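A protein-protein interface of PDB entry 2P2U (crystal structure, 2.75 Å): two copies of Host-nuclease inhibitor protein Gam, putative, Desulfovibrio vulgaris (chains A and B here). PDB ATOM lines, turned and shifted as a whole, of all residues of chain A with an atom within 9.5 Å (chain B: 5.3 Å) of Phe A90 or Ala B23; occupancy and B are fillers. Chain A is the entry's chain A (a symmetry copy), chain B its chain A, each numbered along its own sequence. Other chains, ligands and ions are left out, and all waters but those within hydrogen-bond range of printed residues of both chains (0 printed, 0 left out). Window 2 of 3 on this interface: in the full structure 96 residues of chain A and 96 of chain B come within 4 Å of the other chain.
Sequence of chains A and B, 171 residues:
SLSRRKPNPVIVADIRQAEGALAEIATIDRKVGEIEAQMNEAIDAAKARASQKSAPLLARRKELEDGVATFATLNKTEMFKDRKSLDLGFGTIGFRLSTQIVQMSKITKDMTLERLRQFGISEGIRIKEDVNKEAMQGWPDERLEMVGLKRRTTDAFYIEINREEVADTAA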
ATOM      1  N   ARG A  61     -15.646  -5.976 -22.137  1.00  0.00           N
ATOM      2  CA  ARG A  61     -14.868  -5.010 -22.905  1.00  0.00           C
ATOM      3  C   ARG A  61     -14.891  -5.333 -24.396  1.00  0.00           C
ATOM      4  O   ARG A  61     -14.787  -4.439 -25.193  1.00  0.00           O
ATOM      5  CB  ARG A  61     -13.453  -4.921 -22.390  1.00  0.00           C
ATOM      6  CG  ARG A  61     -12.664  -3.852 -23.038  1.00  0.00           C
ATOM      7  CD  ARG A  61     -11.286  -3.910 -22.496  1.00  0.00           C
ATOM      8  NE  ARG A  61     -10.520  -2.686 -22.702  1.00  0.00           N
ATOM      9  CZ  ARG A  61     -10.083  -2.213 -23.879  1.00  0.00           C
ATOM     10  NH1 ARG A  61      -9.343  -1.099 -23.896  1.00  0.00           N
ATOM     11  NH2 ARG A  61     -10.369  -2.846 -25.021  1.00  0.00           N
ATOM     12  N   LEU A  64     -18.190  -4.206 -26.274  1.00  0.00           N
ATOM     13  CA  LEU A  64     -18.209  -2.747 -26.371  1.00  0.00           C
ATOM     14  C   LEU A  64     -17.244  -2.318 -27.409  1.00  0.00           C
ATOM     15  O   LEU A  64     -17.587  -1.516 -28.274  1.00  0.00           O
ATOM     16  CB  LEU A  64     -17.765  -2.089 -25.073  1.00  0.00           C
ATOM     17  CG  LEU A  64     -18.554  -2.359 -23.811  1.00  0.00           C
ATOM     18  CD1 LEU A  64     -17.724  -1.955 -22.639  1.00  0.00           C
ATOM     19  CD2 LEU A  64     -19.902  -1.655 -23.824  1.00  0.00           C
ATOM     20  N   VAL A  68     -18.593  -0.443 -30.784  1.00  0.00           N
ATOM     21  CA  VAL A  68     -18.184   0.864 -31.294  1.00  0.00           C
ATOM     22  C   VAL A  68     -17.658   0.668 -32.715  1.00  0.00           C
ATOM     23  O   VAL A  68     -17.705   1.583 -33.558  1.00  0.00           O
ATOM     24  CB  VAL A  68     -17.108   1.537 -30.385  1.00  0.00           C
ATOM     25  CG1 VAL A  68     -16.579   2.837 -30.961  1.00  0.00           C
ATOM     26  CG2 VAL A  68     -17.673   1.807 -29.045  1.00  0.00           C
ATOM     27  N   LEU A  86     -12.013  11.022 -34.384  1.00  0.00           N
ATOM     28  CA  LEU A  86     -13.033  11.666 -33.566  1.00  0.00           C
ATOM     29  C   LEU A  86     -12.746  11.547 -32.046  1.00  0.00           C
ATOM     30  O   LEU A  86     -12.779  10.449 -31.505  1.00  0.00           O
ATOM     31  CB  LEU A  86     -14.373  11.030 -33.949  1.00  0.00           C
ATOM     32  CG  LEU A  86     -15.632  11.314 -33.157  1.00  0.00           C
ATOM     33  CD1 LEU A  86     -16.438  12.454 -33.815  1.00  0.00           C
ATOM     34  CD2 LEU A  86     -16.443  10.015 -33.016  1.00  0.00           C
ATOM     35  N   ASP A  87     -12.457  12.664 -31.375  1.00  0.00           N
ATOM     36  CA  ASP A  87     -12.329  12.721 -29.879  1.00  0.00           C
ATOM     37  C   ASP A  87     -13.613  12.455 -29.071  1.00  0.00           C
ATOM     38  O   ASP A  87     -14.626  13.095 -29.311  1.00  0.00           O
ATOM     39  CB  ASP A  87     -11.827  14.085 -29.441  1.00  0.00           C
ATOM     40  CG  ASP A  87     -11.405  14.094 -28.020  1.00  0.00           C
ATOM     41  OD1 ASP A  87     -12.015  13.322 -27.232  1.00  0.00           O
ATOM     42  OD2 ASP A  87     -10.437  14.845 -27.720  1.00  0.00           O
ATOM     43  N   LEU A  88     -13.587  11.537 -28.108  1.00  0.00           N
ATOM     44  CA  LEU A  88     -14.828  11.260 -27.358  1.00  0.00           C
ATOM     45  C   LEU A  88     -14.742  11.613 -25.843  1.00  0.00           C
ATOM     46  O   LEU A  88     -15.502  11.093 -25.014  1.00  0.00           O
ATOM     47  CB  LEU A  88     -15.331   9.830 -27.601  1.00  0.00           C
ATOM     48  CG  LEU A  88     -15.808   9.427 -28.999  1.00  0.00           C
ATOM     49  CD1 LEU A  88     -16.502   8.028 -29.110  1.00  0.00           C
ATOM     50  CD2 LEU A  88     -16.733  10.473 -29.541  1.00  0.00           C
ATOM     51  N   GLY A  89     -13.803  12.506 -25.529  1.00  0.00           N
ATOM     52  CA  GLY A  89     -13.459  12.927 -24.164  1.00  0.00           C
ATOM     53  C   GLY A  89     -12.753  11.887 -23.329  1.00  0.00           C
ATOM     54  O   GLY A  89     -11.676  12.137 -22.751  1.00  0.00           O
ATOM     55  N   PHE A  90     -13.373  10.710 -23.283  1.00  0.00           N
ATOM     56  CA  PHE A  90     -12.835   9.566 -22.569  1.00  0.00           C
ATOM     57  C   PHE A  90     -11.751   8.866 -23.357  1.00  0.00           C
ATOM     58  O   PHE A  90     -10.964   8.085 -22.796  1.00  0.00           O
ATOM     59  CB  PHE A  90     -13.937   8.584 -22.281  1.00  0.00           C
ATOM     60  CG  PHE A  90     -14.763   8.974 -21.149  1.00  0.00           C
ATOM     61  CD1 PHE A  90     -16.153   8.995 -21.271  1.00  0.00           C
ATOM     62  CD2 PHE A  90     -14.156   9.350 -19.944  1.00  0.00           C
ATOM     63  CE1 PHE A  90     -16.946   9.359 -20.181  1.00  0.00           C
ATOM     64  CE2 PHE A  90     -14.912   9.726 -18.852  1.00  0.00           C
ATOM     65  CZ  PHE A  90     -16.328   9.727 -18.958  1.00  0.00           C
ATOM     66  N   GLY A  91     -11.725   9.143 -24.653  1.00  0.00           N
ATOM     67  CA  GLY A  91     -10.596   8.803 -25.472  1.00  0.00           C
ATOM     68  C   GLY A  91     -10.985   8.887 -26.912  1.00  0.00           C
ATOM     69  O   GLY A  91     -12.124   9.195 -27.213  1.00  0.00           O
ATOM     70  N   THR A  92     -10.034   8.609 -27.798  1.00  0.00           N
ATOM     71  CA  THR A  92     -10.239   8.767 -29.226  1.00  0.00           C
ATOM     72  C   THR A  92     -10.638   7.470 -29.919  1.00  0.00           C
ATOM     73  O   THR A  92     -10.246   6.386 -29.498  1.00  0.00           O
ATOM     74  CB  THR A  92      -8.992   9.325 -29.851  1.00  0.00           C
ATOM     75  OG1 THR A  92      -8.746  10.620 -29.293  1.00  0.00           O
ATOM     76  CG2 THR A  92      -9.175   9.440 -31.329  1.00  0.00           C
ATOM     77  N   ILE A  93     -11.460   7.571 -30.951  1.00  0.00           N
ATOM     78  CA  ILE A  93     -11.636   6.446 -31.834  1.00  0.00           C
ATOM     79  C   ILE A  93     -11.209   6.859 -33.215  1.00  0.00           C
ATOM     80  O   ILE A  93     -10.700   7.971 -33.393  1.00  0.00           O
ATOM     81  CB  ILE A  93     -13.037   5.915 -31.894  1.00  0.00           C
ATOM     82  CG1 ILE A  93     -13.975   6.992 -32.435  1.00  0.00           C
ATOM     83  CG2 ILE A  93     -13.442   5.412 -30.574  1.00  0.00           C
ATOM     84  CD1 ILE A  93     -15.263   6.425 -33.015  1.00  0.00           C
ATOM     85  N   ALA B  18     -21.488   6.044 -28.182  1.00  0.00           N
ATOM     86  CA  ALA B  18     -20.113   5.646 -28.283  1.00  0.00           C
ATOM     87  C   ALA B  18     -19.459   6.158 -27.012  1.00  0.00           C
ATOM     88  O   ALA B  18     -19.063   5.365 -26.154  1.00  0.00           O
ATOM     89  CB  ALA B  18     -19.452   6.198 -29.543  1.00  0.00           C
ATOM     90  N   GLU B  19     -19.371   7.475 -26.874  1.00  0.00           N
ATOM     91  CA  GLU B  19     -19.067   8.144 -25.603  1.00  0.00           C
ATOM     92  C   GLU B  19     -19.390   7.300 -24.352  1.00  0.00           C
ATOM     93  O   GLU B  19     -18.575   7.240 -23.460  1.00  0.00           O
ATOM     94  CB  GLU B  19     -19.905   9.400 -25.557  1.00  0.00           C
ATOM     95  CG  GLU B  19     -19.162  10.692 -25.309  1.00  0.00           C
ATOM     96  CD  GLU B  19     -20.069  11.665 -24.511  1.00  0.00           C
ATOM     97  OE1 GLU B  19     -21.184  11.975 -25.017  1.00  0.00           O
ATOM     98  OE2 GLU B  19     -19.689  12.075 -23.379  1.00  0.00           O
ATOM     99  N   GLY B  20     -20.582   6.674 -24.325  1.00  0.00           N
ATOM    100  CA  GLY B  20     -21.061   5.754 -23.297  1.00  0.00           C
ATOM    101  C   GLY B  20     -20.076   4.616 -23.138  1.00  0.00           C
ATOM    102  O   GLY B  20     -19.149   4.674 -22.273  1.00  0.00           O
ATOM    103  N   ALA B  21     -20.240   3.588 -23.983  1.00  0.00           N
ATOM    104  CA  ALA B  21     -19.154   2.571 -24.219  1.00  0.00           C
ATOM    105  C   ALA B  21     -17.697   2.974 -23.808  1.00  0.00           C
ATOM    106  O   ALA B  21     -17.158   2.365 -22.901  1.00  0.00           O
ATOM    107  CB  ALA B  21     -19.186   2.073 -25.657  1.00  0.00           C
ATOM    108  N   LEU B  22     -17.088   4.000 -24.416  1.00  0.00           N
ATOM    109  CA  LEU B  22     -15.716   4.390 -24.023  1.00  0.00           C
ATOM    110  C   LEU B  22     -15.581   4.970 -22.627  1.00  0.00           C
ATOM    111  O   LEU B  22     -14.504   5.484 -22.288  1.00  0.00           O
ATOM    112  CB  LEU B  22     -15.097   5.449 -24.926  1.00  0.00           C
ATOM    113  CG  LEU B  22     -14.901   5.414 -26.425  1.00  0.00           C
ATOM    114  CD1 LEU B  22     -13.679   6.212 -26.716  1.00  0.00           C
ATOM    115  CD2 LEU B  22     -14.734   4.021 -26.918  1.00  0.00           C
ATOM    116  N   ALA B  23     -16.657   5.003 -21.832  1.00  0.00           N
ATOM    117  CA  ALA B  23     -16.498   5.412 -20.425  1.00  0.00           C
ATOM    118  C   ALA B  23     -16.438   4.103 -19.624  1.00  0.00           C
ATOM    119  O   ALA B  23     -15.556   3.930 -18.758  1.00  0.00           O
ATOM    120  CB  ALA B  23     -17.616   6.253 -19.989  1.00  0.00           C
ATOM    121  N   GLU B  24     -17.359   3.191 -19.964  1.00  0.00           N
ATOM    122  CA  GLU B  24     -17.365   1.798 -19.483  1.00  0.00           C
ATOM    123  C   GLU B  24     -16.042   1.037 -19.759  1.00  0.00           C
ATOM    124  O   GLU B  24     -15.348   0.618 -18.825  1.00  0.00           O
ATOM    125  CB  GLU B  24     -18.532   1.043 -20.094  1.00  0.00           C
ATOM    126  CG  GLU B  24     -18.694  -0.355 -19.561  1.00  0.00           C
ATOM    127  CD  GLU B  24     -20.094  -0.843 -19.871  1.00  0.00           C
ATOM    128  OE1 GLU B  24     -20.922   0.058 -20.112  1.00  0.00           O
ATOM    129  OE2 GLU B  24     -20.382  -2.068 -19.896  1.00  0.00           O
ATOM    130  N   ILE B  25     -15.695   0.896 -21.036  1.00  0.00           N
ATOM    131  CA  ILE B  25     -14.389   0.377 -21.403  1.00  0.00           C
ATOM    132  C   ILE B  25     -13.345   0.965 -20.453  1.00  0.00           C
ATOM    133  O   ILE B  25     -12.685   0.204 -19.767  1.00  0.00           O
ATOM    134  CB  ILE B  25     -14.029   0.637 -22.911  1.00  0.00           C
ATOM    135  CG1 ILE B  25     -14.712  -0.389 -23.835  1.00  0.00           C
ATOM    136  CG2 ILE B  25     -12.555   0.692 -23.127  1.00  0.00           C
ATOM    137  CD1 ILE B  25     -15.079   0.138 -25.224  1.00  0.00           C
ATOM    138  N   ALA B  26     -13.230   2.294 -20.359  1.00  0.00           N
ATOM    139  CA  ALA B  26     -12.156   2.898 -19.578  1.00  0.00           C
ATOM    140  C   ALA B  26     -12.337   2.626 -18.109  1.00  0.00           C
ATOM    141  O   ALA B  26     -11.408   2.860 -17.341  1.00  0.00           O
ATOM    142  CB  ALA B  26     -12.029   4.383 -19.830  1.00  0.00           C
ATOM    143  N   THR B  27     -13.514   2.122 -17.719  1.00  0.00           N
ATOM    144  CA  THR B  27     -13.770   1.682 -16.323  1.00  0.00           C
ATOM    145  C   THR B  27     -13.222   0.235 -16.009  1.00  0.00           C
ATOM    146  O   THR B  27     -12.578   0.008 -14.962  1.00  0.00           O
ATOM    147  CB  THR B  27     -15.259   1.899 -15.982  1.00  0.00           C
ATOM    148  OG1 THR B  27     -15.401   3.252 -15.569  1.00  0.00           O
ATOM    149  CG2 THR B  27     -15.795   0.966 -14.863  1.00  0.00           C
ATOM    150  N   ARG B  30      -9.569   0.181 -15.933  1.00  0.00           N
ATOM    151  CA  ARG B  30      -9.122   0.706 -14.657  1.00  0.00           C
ATOM    152  C   ARG B  30      -9.329  -0.355 -13.574  1.00  0.00           C
ATOM    153  O   ARG B  30      -8.514  -0.467 -12.689  1.00  0.00           O
ATOM    154  CB  ARG B  30      -9.884   1.986 -14.334  1.00  0.00           C
ATOM    155  CG  ARG B  30      -9.027   3.172 -13.950  1.00  0.00           C
ATOM    156  CD  ARG B  30      -9.913   4.398 -13.526  1.00  0.00           C
ATOM    157  NE  ARG B  30     -10.194   5.298 -14.646  1.00  0.00           N
ATOM    158  CZ  ARG B  30     -11.378   5.424 -15.208  1.00  0.00           C
ATOM    159  NH1 ARG B  30     -12.425   4.728 -14.744  1.00  0.00           N
ATOM    160  NH2 ARG B  30     -11.509   6.247 -16.238  1.00  0.00           N
ATOM    161  N   ILE B 161      -8.234   4.868 -25.403  1.00  0.00           N
ATOM    162  CA  ILE B 161      -8.391   5.459 -24.050  1.00  0.00           C
ATOM    163  C   ILE B 161      -7.240   6.306 -23.498  1.00  0.00           C
ATOM    164  O   ILE B 161      -6.088   6.039 -23.794  1.00  0.00           O
ATOM    165  CB  ILE B 161      -8.633   4.369 -23.064  1.00  0.00           C
ATOM    166  CG1 ILE B 161      -9.772   3.490 -23.568  1.00  0.00           C
ATOM    167  CG2 ILE B 161      -8.907   4.947 -21.708  1.00  0.00           C
ATOM    168  CD1 ILE B 161     -10.021   2.299 -22.712  1.00  0.00           C
ATOM    169  N   ASN B 162      -7.556   7.313 -22.681  1.00  0.00           N
ATOM    170  CA  ASN B 162      -6.587   8.371 -22.313  1.00  0.00           C
ATOM    171  C   ASN B 162      -5.628   7.941 -21.231  1.00  0.00           C
ATOM    172  O   ASN B 162      -6.005   7.129 -20.389  1.00  0.00           O
ATOM    173  CB  ASN B 162      -7.315   9.639 -21.851  1.00  0.00           C
ATOM    174  CG  ASN B 162      -7.971  10.404 -23.002  1.00  0.00           C
ATOM    175  OD1 ASN B 162      -7.288  11.093 -23.766  1.00  0.00           O
ATOM    176  ND2 ASN B 162      -9.302  10.321 -23.106  1.00  0.00           N
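Among the printed residues, no Asp or Glu carboxylate lies within 4 Å of a Lys or Arg side-chain nitrogen of the other chain.
Arg A61 touches Ile B25 (NH1 to CG2, 3.8 Å). Ile B161 touches Arg A61 (CD1 to NH1, 3.7 Å). CD1 of Leu A64 touches CG of Glu B24, at 3.6 Å. Leu A64 touches Ile B25 (CB to CD1, 3.5 Å). CG2 of Val A68 touches CB of Ala B21, 3.7 Å away. Glu B19 touches Leu A88 (N to CD1, 3.7 Å). Phe A90 touches Leu B22 (CB to O, 3.2 Å). CE1 of Phe A90 touches CB of Ala B23, at 3.2 Å. Phe A90 touches Ile B161. Ile A93 touches Leu B22 (CG2 to CD1, 3.9 Å).
Leu A86 touches none of the printed residues of chain B. Of the printed residues of chain B, Leu A88 touches Ala B18 and Glu B19. Printed residues of chain B within 4 Å of Gly A89: Asn B162 (3.0 Å). Phe A90 touches just these residues of chain B: Glu B19, Leu B22, Ala B23, Ile B161 and Asn B162. No residue of chain A comes within 4 Å of Gly B20. Ala B21 touches one residue of chain A. Printed residues of chain A within 4 Å of Leu B22: Phe A90, Gly A91 and Ile A93. Ala B23 touches just one residue of chain A: Phe A90. Ala B26 touches none of the printed residues of chain A. Thr B27 touches none of the printed residues of chain A. The nearest residue of chain A that does not touch Ala B23 is Leu A64 (6.9 Å).
No position is printed for both chains.
The side-chain hydroxyl of Thr B27 sits at hydrogen-bond distance from the backbone carbonyl oxygen of Ala B23 (3.3 Å). The backbone carbonyl oxygen (O) of Leu A86 sits at hydrogen-bond distance from the backbone NH (N) of Ile A93 (3.2 Å). The side-chain carboxylate of Asp A87 sits at hydrogen-bond distance from the backbone NH of Gly A89 (2.6 Å).
The side-chain amide nitrogen (ND2) of Asn B162 is in hydrogen-bond range of the backbone carbonyl oxygen (O) of Gly A89, at 3.0 Å. ND2 of Asn B162 is in hydrogen-bond range of O of Phe A90 (2.8 Å). The backbone NH of Gly A91 lies close to the side-chain amide nitrogen of Asn B162, at 3.1 Å.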
